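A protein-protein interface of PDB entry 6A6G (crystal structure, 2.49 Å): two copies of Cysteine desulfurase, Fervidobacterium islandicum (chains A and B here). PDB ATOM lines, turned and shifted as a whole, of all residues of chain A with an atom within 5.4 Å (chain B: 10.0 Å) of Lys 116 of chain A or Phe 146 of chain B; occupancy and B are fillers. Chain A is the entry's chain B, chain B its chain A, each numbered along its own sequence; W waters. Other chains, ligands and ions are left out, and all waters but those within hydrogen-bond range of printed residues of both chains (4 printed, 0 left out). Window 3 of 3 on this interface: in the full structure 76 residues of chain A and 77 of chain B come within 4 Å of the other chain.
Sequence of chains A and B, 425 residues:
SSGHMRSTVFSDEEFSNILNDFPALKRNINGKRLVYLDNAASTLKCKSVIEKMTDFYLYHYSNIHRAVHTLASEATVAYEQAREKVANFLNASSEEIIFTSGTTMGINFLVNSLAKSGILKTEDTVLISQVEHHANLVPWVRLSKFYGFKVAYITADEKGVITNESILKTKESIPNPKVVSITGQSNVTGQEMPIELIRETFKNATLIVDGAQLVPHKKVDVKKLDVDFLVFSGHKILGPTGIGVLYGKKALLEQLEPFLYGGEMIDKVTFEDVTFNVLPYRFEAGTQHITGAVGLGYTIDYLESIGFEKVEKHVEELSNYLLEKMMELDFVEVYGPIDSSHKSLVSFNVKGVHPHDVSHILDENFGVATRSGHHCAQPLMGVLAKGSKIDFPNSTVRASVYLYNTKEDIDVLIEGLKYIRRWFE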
ATOM      1  N   VAL A 111       4.889  -2.089 -13.663  1.00  0.00           N
ATOM      2  CA  VAL A 111       4.773  -0.689 -14.073  1.00  0.00           C
ATOM      3  C   VAL A 111       5.127   0.228 -12.901  1.00  0.00           C
ATOM      4  O   VAL A 111       5.955   1.126 -13.034  1.00  0.00           O
ATOM      5  CB  VAL A 111       3.386  -0.322 -14.568  1.00  0.00           C
ATOM      6  CG1 VAL A 111       3.383   1.125 -15.056  1.00  0.00           C
ATOM      7  CG2 VAL A 111       2.924  -1.272 -15.660  1.00  0.00           C
ATOM      8  N   ASN A 112       4.527  -0.021 -11.742  1.00  0.00           N
ATOM      9  CA  ASN A 112       4.738   0.855 -10.603  1.00  0.00           C
ATOM     10  C   ASN A 112       6.178   0.823 -10.122  1.00  0.00           C
ATOM     11  O   ASN A 112       6.829   1.853  -9.935  1.00  0.00           O
ATOM     12  CB  ASN A 112       3.781   0.496  -9.461  1.00  0.00           C
ATOM     13  CG  ASN A 112       2.386   0.968  -9.741  1.00  0.00           C
ATOM     14  OD1 ASN A 112       2.147   2.178  -9.702  1.00  0.00           O
ATOM     15  ND2 ASN A 112       1.467   0.040 -10.117  1.00  0.00           N
ATOM     16  N   SER A 113       6.656  -0.383  -9.907  1.00  0.00           N
ATOM     17  CA  SER A 113       7.942  -0.582  -9.332  1.00  0.00           C
ATOM     18  C   SER A 113       9.000  -0.117 -10.317  1.00  0.00           C
ATOM     19  O   SER A 113       9.950   0.541  -9.918  1.00  0.00           O
ATOM     20  CB  SER A 113       8.124  -2.042  -8.948  1.00  0.00           C
ATOM     21  OG  SER A 113       9.438  -2.270  -8.490  1.00  0.00           O
ATOM     22  N   LEU A 114       8.854  -0.416 -11.598  1.00  0.00           N
ATOM     23  CA  LEU A 114       9.835   0.108 -12.556  1.00  0.00           C
ATOM     24  C   LEU A 114       9.859   1.659 -12.510  1.00  0.00           C
ATOM     25  O   LEU A 114      10.936   2.249 -12.515  1.00  0.00           O
ATOM     26  CB  LEU A 114       9.627  -0.403 -13.999  1.00  0.00           C
ATOM     27  CG  LEU A 114      10.032  -1.851 -14.203  1.00  0.00           C
ATOM     28  CD1 LEU A 114       9.380  -2.439 -15.446  1.00  0.00           C
ATOM     29  CD2 LEU A 114      11.529  -2.020 -14.302  1.00  0.00           C
ATOM     30  N   ALA A 115       8.699   2.302 -12.457  1.00  0.00           N
ATOM     31  CA  ALA A 115       8.657   3.743 -12.325  1.00  0.00           C
ATOM     32  C   ALA A 115       9.215   4.231 -10.965  1.00  0.00           C
ATOM     33  O   ALA A 115      10.074   5.107 -10.927  1.00  0.00           O
ATOM     34  CB  ALA A 115       7.253   4.257 -12.554  1.00  0.00           C
ATOM     35  N   LYS A 116       8.770   3.648  -9.857  1.00  0.00           N
ATOM     36  CA  LYS A 116       9.256   4.087  -8.536  1.00  0.00           C
ATOM     37  C   LYS A 116      10.755   3.808  -8.348  1.00  0.00           C
ATOM     38  O   LYS A 116      11.350   4.422  -7.488  1.00  0.00           O
ATOM     39  CB  LYS A 116       8.481   3.420  -7.379  1.00  0.00           C
ATOM     40  CG  LYS A 116       7.157   4.077  -6.989  1.00  0.00           C
ATOM     41  CD  LYS A 116       6.576   3.446  -5.722  1.00  0.00           C
ATOM     42  CE  LYS A 116       6.279   1.928  -5.838  1.00  0.00           C
ATOM     43  NZ  LYS A 116       5.725   1.285  -4.576  1.00  0.00           N
ATOM     44  N   SER A 117      11.335   2.866  -9.108  1.00  0.00           N
ATOM     45  CA  SER A 117      12.756   2.499  -8.978  1.00  0.00           C
ATOM     46  C   SER A 117      13.671   3.363  -9.866  1.00  0.00           C
ATOM     47  O   SER A 117      14.905   3.242  -9.802  1.00  0.00           O
ATOM     48  CB  SER A 117      13.014   1.045  -9.377  1.00  0.00           C
ATOM     49  OG  SER A 117      12.271   0.110  -8.633  1.00  0.00           O
ATOM     50  N   GLY A 118      13.075   4.200 -10.704  1.00  0.00           N
ATOM     51  CA  GLY A 118      13.838   5.080 -11.555  1.00  0.00           C
ATOM     52  C   GLY A 118      14.437   4.425 -12.792  1.00  0.00           C
ATOM     53  O   GLY A 118      15.369   4.959 -13.383  1.00  0.00           O
ATOM     54  N   TYR A 147       3.173   8.916 -14.085  1.00  0.00           N
ATOM     55  CA  TYR A 147       4.618   8.868 -14.038  1.00  0.00           C
ATOM     56  C   TYR A 147       5.278   9.508 -15.250  1.00  0.00           C
ATOM     57  O   TYR A 147       6.497   9.528 -15.307  1.00  0.00           O
ATOM     58  CB  TYR A 147       5.089   7.419 -13.992  1.00  0.00           C
ATOM     59  CG  TYR A 147       4.743   6.666 -12.758  1.00  0.00           C
ATOM     60  CD1 TYR A 147       5.226   7.061 -11.519  1.00  0.00           C
ATOM     61  CD2 TYR A 147       3.983   5.512 -12.830  1.00  0.00           C
ATOM     62  CE1 TYR A 147       4.922   6.345 -10.362  1.00  0.00           C
ATOM     63  CE2 TYR A 147       3.672   4.785 -11.695  1.00  0.00           C
ATOM     64  CZ  TYR A 147       4.140   5.203 -10.461  1.00  0.00           C
ATOM     65  OH  TYR A 147       3.815   4.469  -9.349  1.00  0.00           O
ATOM     66  N   GLU A 257      12.306  -1.291  -6.327  1.00  0.00           N
ATOM     67  CA  GLU A 257      11.474  -0.902  -5.186  1.00  0.00           C
ATOM     68  C   GLU A 257      10.340  -1.903  -5.077  1.00  0.00           C
ATOM     69  O   GLU A 257       9.643  -2.170  -6.059  1.00  0.00           O
ATOM     70  CB  GLU A 257      10.852   0.475  -5.415  1.00  0.00           C
ATOM     71  CG  GLU A 257       9.944   0.977  -4.271  1.00  0.00           C
ATOM     72  CD  GLU A 257      10.701   1.350  -2.999  1.00  0.00           C
ATOM     73  OE1 GLU A 257      11.939   1.377  -3.043  1.00  0.00           O
ATOM     74  OE2 GLU A 257      10.085   1.588  -1.950  1.00  0.00           O
ATOM     75  N   PRO A 258      10.126  -2.457  -3.893  1.00  0.00           N
ATOM     76  CA  PRO A 258       8.935  -3.311  -3.808  1.00  0.00           C
ATOM     77  C   PRO A 258       7.655  -2.553  -4.164  1.00  0.00           C
ATOM     78  O   PRO A 258       7.532  -1.317  -3.970  1.00  0.00           O
ATOM     79  CB  PRO A 258       8.877  -3.750  -2.340  1.00  0.00           C
ATOM     80  CG  PRO A 258      10.196  -3.416  -1.764  1.00  0.00           C
ATOM     81  CD  PRO A 258      10.967  -2.521  -2.701  1.00  0.00           C
ATOM     82  N   PHE A 259       6.725  -3.320  -4.697  1.00  0.00           N
ATOM     83  CA  PHE A 259       5.428  -2.819  -5.043  1.00  0.00           C
ATOM     84  C   PHE A 259       4.581  -2.688  -3.788  1.00  0.00           C
ATOM     85  O   PHE A 259       4.108  -1.619  -3.484  1.00  0.00           O
ATOM     86  CB  PHE A 259       4.765  -3.735  -6.093  1.00  0.00           C
ATOM     87  CG  PHE A 259       3.426  -3.269  -6.529  1.00  0.00           C
ATOM     88  CD1 PHE A 259       3.140  -1.919  -6.613  1.00  0.00           C
ATOM     89  CD2 PHE A 259       2.441  -4.193  -6.858  1.00  0.00           C
ATOM     90  CE1 PHE A 259       1.874  -1.492  -7.011  1.00  0.00           C
ATOM     91  CE2 PHE A 259       1.179  -3.775  -7.276  1.00  0.00           C
ATOM     92  CZ  PHE A 259       0.895  -2.430  -7.348  1.00  0.00           C
ATOM     93  N   TYR A 261       3.952  -3.117   0.435  1.00  0.00           N
ATOM     94  CA  TYR A 261       4.674  -3.088   1.679  1.00  0.00           C
ATOM     95  C   TYR A 261       3.873  -3.725   2.799  1.00  0.00           C
ATOM     96  O   TYR A 261       2.655  -3.649   2.827  1.00  0.00           O
ATOM     97  CB  TYR A 261       5.018  -1.651   2.055  1.00  0.00           C
ATOM     98  CG  TYR A 261       5.708  -0.887   0.955  1.00  0.00           C
ATOM     99  CD1 TYR A 261       7.082  -1.025   0.733  1.00  0.00           C
ATOM    100  CD2 TYR A 261       5.002  -0.021   0.143  1.00  0.00           C
ATOM    101  CE1 TYR A 261       7.718  -0.323  -0.280  1.00  0.00           C
ATOM    102  CE2 TYR A 261       5.624   0.691  -0.861  1.00  0.00           C
ATOM    103  CZ  TYR A 261       6.993   0.541  -1.071  1.00  0.00           C
ATOM    104  OH  TYR A 261       7.612   1.251  -2.091  1.00  0.00           O
ATOM    105  N   ASN B 108      -2.448  -1.244   1.266  1.00  0.00           N
ATOM    106  CA  ASN B 108      -1.637  -0.689   0.142  1.00  0.00           C
ATOM    107  C   ASN B 108      -2.515  -0.035  -0.901  1.00  0.00           C
ATOM    108  O   ASN B 108      -2.182   1.039  -1.373  1.00  0.00           O
ATOM    109  CB  ASN B 108      -0.767  -1.769  -0.523  1.00  0.00           C
ATOM    110  CG  ASN B 108       0.502  -2.047   0.261  1.00  0.00           C
ATOM    111  OD1 ASN B 108       1.583  -1.461   0.000  1.00  0.00           O
ATOM    112  ND2 ASN B 108       0.383  -2.902   1.254  1.00  0.00           N
ATOM    113  N   VAL B 111      -3.508   3.483   0.504  1.00  0.00           N
ATOM    114  CA  VAL B 111      -2.470   4.492   0.522  1.00  0.00           C
ATOM    115  C   VAL B 111      -2.262   5.013  -0.878  1.00  0.00           C
ATOM    116  O   VAL B 111      -2.243   6.229  -1.124  1.00  0.00           O
ATOM    117  CB  VAL B 111      -1.090   3.949   1.029  1.00  0.00           C
ATOM    118  CG1 VAL B 111      -0.098   5.086   1.160  1.00  0.00           C
ATOM    119  CG2 VAL B 111      -1.187   3.209   2.376  1.00  0.00           C
ATOM    120  N   ASN B 112      -2.059   4.087  -1.800  1.00  0.00           N
ATOM    121  CA  ASN B 112      -1.828   4.436  -3.194  1.00  0.00           C
ATOM    122  C   ASN B 112      -3.002   5.182  -3.808  1.00  0.00           C
ATOM    123  O   ASN B 112      -2.815   6.221  -4.389  1.00  0.00           O
ATOM    124  CB  ASN B 112      -1.437   3.195  -4.020  1.00  0.00           C
ATOM    125  CG  ASN B 112      -0.019   2.753  -3.725  1.00  0.00           C
ATOM    126  OD1 ASN B 112       0.956   3.445  -4.118  1.00  0.00           O
ATOM    127  ND2 ASN B 112       0.126   1.647  -2.987  1.00  0.00           N
ATOM    128  N   ALA B 115      -3.596   8.684  -2.370  1.00  0.00           N
ATOM    129  CA  ALA B 115      -2.602   9.621  -2.908  1.00  0.00           C
ATOM    130  C   ALA B 115      -2.823   9.950  -4.385  1.00  0.00           C
ATOM    131  O   ALA B 115      -2.683  11.113  -4.790  1.00  0.00           O
ATOM    132  CB  ALA B 115      -1.195   9.081  -2.707  1.00  0.00           C
ATOM    133  N   LYS B 116      -3.136   8.936  -5.196  1.00  0.00           N
ATOM    134  CA  LYS B 116      -3.341   9.135  -6.647  1.00  0.00           C
ATOM    135  C   LYS B 116      -4.624   9.939  -6.918  1.00  0.00           C
ATOM    136  O   LYS B 116      -4.728  10.614  -7.928  1.00  0.00           O
ATOM    137  CB  LYS B 116      -3.393   7.789  -7.396  1.00  0.00           C
ATOM    138  CG  LYS B 116      -2.039   7.120  -7.674  1.00  0.00           C
ATOM    139  CD  LYS B 116      -2.119   6.058  -8.767  1.00  0.00           C
ATOM    140  CE  LYS B 116      -3.068   4.892  -8.407  1.00  0.00           C
ATOM    141  NZ  LYS B 116      -2.961   3.660  -9.289  1.00  0.00           N
ATOM    142  N   LEU B 120      -4.816  12.508  -0.311  1.00  0.00           N
ATOM    143  CA  LEU B 120      -3.719  12.464   0.610  1.00  0.00           C
ATOM    144  C   LEU B 120      -2.536  13.082  -0.069  1.00  0.00           C
ATOM    145  O   LEU B 120      -1.812  12.416  -0.763  1.00  0.00           O
ATOM    146  CB  LEU B 120      -3.473  11.017   0.977  1.00  0.00           C
ATOM    147  CG  LEU B 120      -2.511  10.775   2.097  1.00  0.00           C
ATOM    148  CD1 LEU B 120      -2.949  11.568   3.313  1.00  0.00           C
ATOM    149  CD2 LEU B 120      -2.443   9.291   2.390  1.00  0.00           C
ATOM    150  N   LYS B 121      -2.327  14.372   0.155  1.00  0.00           N
ATOM    151  CA  LYS B 121      -1.347  15.157  -0.627  1.00  0.00           C
ATOM    152  C   LYS B 121      -0.155  15.548   0.231  1.00  0.00           C
ATOM    153  O   LYS B 121      -0.137  15.292   1.427  1.00  0.00           O
ATOM    154  CB  LYS B 121      -2.002  16.393  -1.293  1.00  0.00           C
ATOM    155  CG  LYS B 121      -3.225  16.930  -0.536  1.00  0.00           C
ATOM    156  CD  LYS B 121      -4.210  17.722  -1.389  1.00  0.00           C
ATOM    157  CE  LYS B 121      -5.631  17.563  -0.849  1.00  0.00           C
ATOM    158  NZ  LYS B 121      -6.493  18.739  -1.166  1.00  0.00           N
ATOM    159  N   THR B 122       0.848  16.126  -0.412  1.00  0.00           N
ATOM    160  CA  THR B 122       2.012  16.715   0.251  1.00  0.00           C
ATOM    161  C   THR B 122       1.746  17.367   1.616  1.00  0.00           C
ATOM    162  O   THR B 122       2.391  17.012   2.604  1.00  0.00           O
ATOM    163  CB  THR B 122       2.641  17.769  -0.668  1.00  0.00           C
ATOM    164  OG1 THR B 122       2.970  17.152  -1.920  1.00  0.00           O
ATOM    165  CG2 THR B 122       3.900  18.371  -0.042  1.00  0.00           C
ATOM    166  N   VAL B 138       4.105   0.153   7.644  1.00  0.00           N
ATOM    167  CA  VAL B 138       5.122   0.278   6.623  1.00  0.00           C
ATOM    168  C   VAL B 138       4.687   0.964   5.320  1.00  0.00           C
ATOM    169  O   VAL B 138       5.485   1.682   4.745  1.00  0.00           O
ATOM    170  CB  VAL B 138       5.814  -1.066   6.284  1.00  0.00           C
ATOM    171  CG1 VAL B 138       6.946  -0.829   5.277  1.00  0.00           C
ATOM    172  CG2 VAL B 138       6.388  -1.689   7.530  1.00  0.00           C
ATOM    173  N   PRO B 139       3.442   0.758   4.845  1.00  0.00           N
ATOM    174  CA  PRO B 139       3.017   1.447   3.620  1.00  0.00           C
ATOM    175  C   PRO B 139       2.925   2.949   3.759  1.00  0.00           C
ATOM    176  O   PRO B 139       3.264   3.672   2.810  1.00  0.00           O
ATOM    177  CB  PRO B 139       1.628   0.895   3.356  1.00  0.00           C
ATOM    178  CG  PRO B 139       1.617  -0.400   3.987  1.00  0.00           C
ATOM    179  CD  PRO B 139       2.507  -0.307   5.195  1.00  0.00           C
ATOM    180  N   TRP B 140       2.451   3.411   4.913  1.00  0.00           N
ATOM    181  CA  TRP B 140       2.307   4.826   5.149  1.00  0.00           C
ATOM    182  C   TRP B 140       3.711   5.434   5.219  1.00  0.00           C
ATOM    183  O   TRP B 140       4.021   6.441   4.553  1.00  0.00           O
ATOM    184  CB  TRP B 140       1.532   5.124   6.440  1.00  0.00           C
ATOM    185  CG  TRP B 140       0.164   4.533   6.491  1.00  0.00           C
ATOM    186  CD1 TRP B 140      -0.216   3.462   7.211  1.00  0.00           C
ATOM    187  CD2 TRP B 140      -0.987   4.964   5.771  1.00  0.00           C
ATOM    188  NE1 TRP B 140      -1.542   3.179   6.989  1.00  0.00           N
ATOM    189  CE2 TRP B 140      -2.043   4.101   6.119  1.00  0.00           C
ATOM    190  CE3 TRP B 140      -1.241   6.010   4.888  1.00  0.00           C
ATOM    191  CZ2 TRP B 140      -3.340   4.253   5.606  1.00  0.00           C
ATOM    192  CZ3 TRP B 140      -2.505   6.159   4.393  1.00  0.00           C
ATOM    193  CH2 TRP B 140      -3.547   5.294   4.755  1.00  0.00           C
ATOM    194  N   VAL B 141       4.574   4.802   5.984  1.00  0.00           N
ATOM    195  CA  VAL B 141       5.901   5.361   6.208  1.00  0.00           C
ATOM    196  C   VAL B 141       6.688   5.378   4.911  1.00  0.00           C
ATOM    197  O   VAL B 141       7.196   6.406   4.532  1.00  0.00           O
ATOM    198  CB  VAL B 141       6.636   4.608   7.309  1.00  0.00           C
ATOM    199  CG1 VAL B 141       8.054   5.103   7.443  1.00  0.00           C
ATOM    200  CG2 VAL B 141       5.901   4.772   8.630  1.00  0.00           C
ATOM    201  N   ARG B 142       6.714   4.265   4.180  1.00  0.00           N
ATOM    202  CA  ARG B 142       7.494   4.193   2.951  1.00  0.00           C
ATOM    203  C   ARG B 142       6.956   5.072   1.855  1.00  0.00           C
ATOM    204  O   ARG B 142       7.718   5.787   1.204  1.00  0.00           O
ATOM    205  CB  ARG B 142       7.576   2.776   2.420  1.00  0.00           C
ATOM    206  CG  ARG B 142       8.503   2.634   1.224  1.00  0.00           C
ATOM    207  CD  ARG B 142       9.914   3.037   1.591  1.00  0.00           C
ATOM    208  NE  ARG B 142      10.818   3.016   0.441  1.00  0.00           N
ATOM    209  CZ  ARG B 142      12.151   3.001   0.527  1.00  0.00           C
ATOM    210  NH1 ARG B 142      12.752   2.963   1.710  1.00  0.00           N
ATOM    211  NH2 ARG B 142      12.895   2.960  -0.573  1.00  0.00           N
ATOM    212  N   LEU B 143       5.648   5.000   1.624  1.00  0.00           N
ATOM    213  CA  LEU B 143       5.037   5.833   0.600  1.00  0.00           C
ATOM    214  C   LEU B 143       5.000   7.330   0.932  1.00  0.00           C
ATOM    215  O   LEU B 143       4.753   8.123   0.043  1.00  0.00           O
ATOM    216  CB  LEU B 143       3.649   5.313   0.237  1.00  0.00           C
ATOM    217  CG  LEU B 143       3.722   3.985  -0.508  1.00  0.00           C
ATOM    218  CD1 LEU B 143       2.402   3.234  -0.489  1.00  0.00           C
ATOM    219  CD2 LEU B 143       4.156   4.269  -1.925  1.00  0.00           C
ATOM    220  N   SER B 144       5.222   7.724   2.183  1.00  0.00           N
ATOM    221  CA  SER B 144       5.404   9.155   2.500  1.00  0.00           C
ATOM    222  C   SER B 144       6.562   9.754   1.673  1.00  0.00           C
ATOM    223  O   SER B 144       6.444  10.867   1.185  1.00  0.00           O
ATOM    224  CB  SER B 144       5.671   9.372   3.988  1.00  0.00           C
ATOM    225  OG  SER B 144       6.798   8.624   4.391  1.00  0.00           O
ATOM    226  N   LYS B 145       7.640   8.988   1.489  1.00  0.00           N
ATOM    227  CA  LYS B 145       8.786   9.419   0.673  1.00  0.00           C
ATOM    228  C   LYS B 145       8.391   9.688  -0.771  1.00  0.00           C
ATOM    229  O   LYS B 145       8.915  10.605  -1.370  1.00  0.00           O
ATOM    230  CB  LYS B 145       9.940   8.387   0.664  1.00  0.00           C
ATOM    231  CG  LYS B 145      10.479   7.938   2.025  1.00  0.00           C
ATOM    232  CD  LYS B 145      10.904   9.082   2.970  1.00  0.00           C
ATOM    233  CE  LYS B 145      10.457   8.812   4.412  1.00  0.00           C
ATOM    234  NZ  LYS B 145      10.726   7.408   4.899  1.00  0.00           N
ATOM    235  N   PHE B 146       7.484   8.892  -1.333  1.00  0.00           N
ATOM    236  CA  PHE B 146       7.065   9.055  -2.732  1.00  0.00           C
ATOM    237  C   PHE B 146       5.985  10.093  -2.910  1.00  0.00           C
ATOM    238  O   PHE B 146       5.989  10.763  -3.895  1.00  0.00           O
ATOM    239  CB  PHE B 146       6.621   7.729  -3.334  1.00  0.00           C
ATOM    240  CG  PHE B 146       7.734   6.735  -3.471  1.00  0.00           C
ATOM    241  CD1 PHE B 146       8.550   6.734  -4.597  1.00  0.00           C
ATOM    242  CD2 PHE B 146       7.983   5.825  -2.473  1.00  0.00           C
ATOM    243  CE1 PHE B 146       9.583   5.822  -4.742  1.00  0.00           C
ATOM    244  CE2 PHE B 146       9.019   4.929  -2.592  1.00  0.00           C
ATOM    245  CZ  PHE B 146       9.822   4.923  -3.736  1.00  0.00           C
ATOM    246  N   TYR B 147       5.060  10.249  -1.974  1.00  0.00           N
ATOM    247  CA  TYR B 147       3.967  11.213  -2.159  1.00  0.00           C
ATOM    248  C   TYR B 147       4.028  12.451  -1.245  1.00  0.00           C
ATOM    249  O   TYR B 147       3.266  13.398  -1.436  1.00  0.00           O
ATOM    250  CB  TYR B 147       2.627  10.523  -1.957  1.00  0.00           C
ATOM    251  CG  TYR B 147       2.329   9.429  -2.932  1.00  0.00           C
ATOM    252  CD1 TYR B 147       2.122   9.699  -4.286  1.00  0.00           C
ATOM    253  CD2 TYR B 147       2.198   8.112  -2.499  1.00  0.00           C
ATOM    254  CE1 TYR B 147       1.815   8.670  -5.185  1.00  0.00           C
ATOM    255  CE2 TYR B 147       1.894   7.081  -3.384  1.00  0.00           C
ATOM    256  CZ  TYR B 147       1.692   7.354  -4.720  1.00  0.00           C
ATOM    257  OH  TYR B 147       1.373   6.304  -5.571  1.00  0.00           O
ATOM    258  N   GLY B 148       4.874  12.430  -0.226  1.00  0.00           N
ATOM    259  CA  GLY B 148       5.146  13.640   0.583  1.00  0.00           C
ATOM    260  C   GLY B 148       4.179  14.005   1.694  1.00  0.00           C
ATOM    261  O   GLY B 148       4.289  15.084   2.243  1.00  0.00           O
ATOM    262  N   PHE B 149       3.227  13.129   2.017  1.00  0.00           N
ATOM    263  CA  PHE B 149       2.311  13.345   3.156  1.00  0.00           C
ATOM    264  C   PHE B 149       3.053  13.028   4.416  1.00  0.00           C
ATOM    265  O   PHE B 149       4.047  12.321   4.377  1.00  0.00           O
ATOM    266  CB  PHE B 149       1.014  12.463   3.053  1.00  0.00           C
ATOM    267  CG  PHE B 149       1.258  10.964   2.953  1.00  0.00           C
ATOM    268  CD1 PHE B 149       1.567  10.207   4.081  1.00  0.00           C
ATOM    269  CD2 PHE B 149       1.182  10.321   1.745  1.00  0.00           C
ATOM    270  CE1 PHE B 149       1.805   8.837   3.996  1.00  0.00           C
ATOM    271  CE2 PHE B 149       1.409   8.962   1.640  1.00  0.00           C
ATOM    272  CZ  PHE B 149       1.718   8.216   2.762  1.00  0.00           C
ATOM    273  N   LYS B 150       2.553  13.505   5.540  1.00  0.00           N
ATOM    274  CA  LYS B 150       3.222  13.282   6.818  1.00  0.00           C
ATOM    275  C   LYS B 150       2.613  12.110   7.553  1.00  0.00           C
ATOM    276  O   LYS B 150       1.431  11.821   7.411  1.00  0.00           O
ATOM    277  CB  LYS B 150       3.141  14.530   7.736  1.00  0.00           C
ATOM    278  CG  LYS B 150       3.559  15.855   7.112  1.00  0.00           C
ATOM    279  CD  LYS B 150       4.800  15.771   6.222  1.00  0.00           C
ATOM    280  CE  LYS B 150       6.071  15.349   6.954  1.00  0.00           C
ATOM    281  NZ  LYS B 150       7.031  14.658   6.032  1.00  0.00           N
ATOM    282  N   VAL B 151       3.419  11.466   8.384  1.00  0.00           N
ATOM    283  CA  VAL B 151       2.939  10.387   9.196  1.00  0.00           C
ATOM    284  C   VAL B 151       3.061  10.782  10.659  1.00  0.00           C
ATOM    285  O   VAL B 151       4.117  11.186  11.092  1.00  0.00           O
ATOM    286  CB  VAL B 151       3.740   9.132   8.907  1.00  0.00           C
ATOM    287  CG1 VAL B 151       3.322   8.000   9.848  1.00  0.00           C
ATOM    288  CG2 VAL B 151       3.541   8.749   7.458  1.00  0.00           C
ATOM    289  N   PHE B 259      -6.539   1.250  -7.742  1.00  0.00           N
ATOM    290  CA  PHE B 259      -5.200   0.887  -7.441  1.00  0.00           C
ATOM    291  C   PHE B 259      -4.622   0.040  -8.551  1.00  0.00           C
ATOM    292  O   PHE B 259      -3.541   0.380  -9.093  1.00  0.00           O
ATOM    293  CB  PHE B 259      -5.158   0.105  -6.130  1.00  0.00           C
ATOM    294  CG  PHE B 259      -3.796  -0.363  -5.726  1.00  0.00           C
ATOM    295  CD1 PHE B 259      -2.668   0.402  -5.946  1.00  0.00           C
ATOM    296  CD2 PHE B 259      -3.650  -1.587  -5.109  1.00  0.00           C
ATOM    297  CE1 PHE B 259      -1.420  -0.059  -5.562  1.00  0.00           C
ATOM    298  CE2 PHE B 259      -2.401  -2.051  -4.731  1.00  0.00           C
ATOM    299  CZ  PHE B 259      -1.297  -1.289  -4.941  1.00  0.00           C
HETATM  300  O   HOH W   1       2.222  -0.006  -2.212  1.00  0.00           O
HETATM  301  O   HOH W   2       3.270   2.320  -5.403  1.00  0.00           O
HETATM  302  O   HOH W   3      -1.305  -0.211 -10.580  1.00  0.00           O
HETATM  303  O   HOH W   4       4.181   5.144  -6.297  1.00  0.00           O
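O of Tyr 261 of chain A sits at hydrogen-bond distance from ND2 of Asn 108 of chain B, at 2.9 Å.
The guanidinium group (NE) of Arg 142 of chain B is in salt-bridge range of the side-chain carboxylate (OE2) of Glu 257 of chain A, at 2.9 Å.
The backbone carbonyl oxygen (O) of Asn 108 of chain B lies within hydrogen-bond range of the side-chain amide nitrogen (ND2) of Asn 112 of chain B, 2.9 Å away.
OE2 of Glu 257 of chain A is in hydrogen-bond range of OH of Tyr 261 of chain A, at 2.5 Å.
Among the printed residues, pairs that only touch across the chains: Tyr 261 of chain A with Arg 142 of chain B, Phe 259 of chain A with Phe 259 of chain B, Lys 116 of chain A with Phe 146 of chain B, Glu 257 of chain A with Phe 146 of chain B, Tyr 261 of chain A with Pro 139 of chain B, Tyr 261 of chain A with Leu 143 of chain B, Tyr 261 of chain A with Val 138 of chain B and Tyr 261 of chain A with Phe 146 of chain B.
Of the printed residues of chain A, Phe 146 of chain B touches Lys 116 (3.6 Å), Glu 257 (3.6 Å) and Tyr 261 (3.97 Å).
No residue of chain B comes within 4 Å of Ser 113 of chain A.
No residue of chain B comes within 4 Å of Ala 115 of chain A.
No residue of chain B comes within 4 Å of Ser 117 of chain A.
Printed residues of chain A within 4 Å of Phe 259 of chain B: Phe 259 (3.4 Å).
Printed residues of chain A within 4 Å of Arg 142 of chain B: Glu 257 and Tyr 261.
The nearest residue of chain B that does not touch Lys 116 of chain A is Leu 143 of chain B (4.3 Å).
The nearest printed residue of chain B that does not touch Phe 259 of chain A is Asn 108 of chain B (4.3 Å).
Of the 13 printed residues of chain A, 4 touch a printed residue of chain B.
Hydrophobic or aromatic side chains of chain A that line the printed part of chain B: Phe 259 and Tyr 261.
Of the 23 printed residues of chain B, 7 touch a printed residue of chain A.
Hydrophobic or aromatic side chains of chain B within 4 Å of the printed part of chain A: Val 138, Pro 139, Leu 143, Phe 146 and Phe 259.
Among the printed residues, Asp or Glu carboxylates within 4 Å of a Lys or Arg side-chain nitrogen of the other chain: Glu 257 of chain A with Arg 142 of chain B (2.9 Å).
Phe 259 of chain A touches its own counterpart, Phe 259 of chain B.
Positions printed for both chains: 111, 112, 115, 116, 147 and 259.
Of the 10 pairs that touch across the chains among the printed residues, 1 has its exchanged pair printed and touching as well.
Water W1 lies within hydrogen-bond range of OD1 of Asn 108 of chain B (2.7 Å), ND2 of Asn 112 of chain B (2.8 Å) and O of Phe 259 of chain A (2.8 Å).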
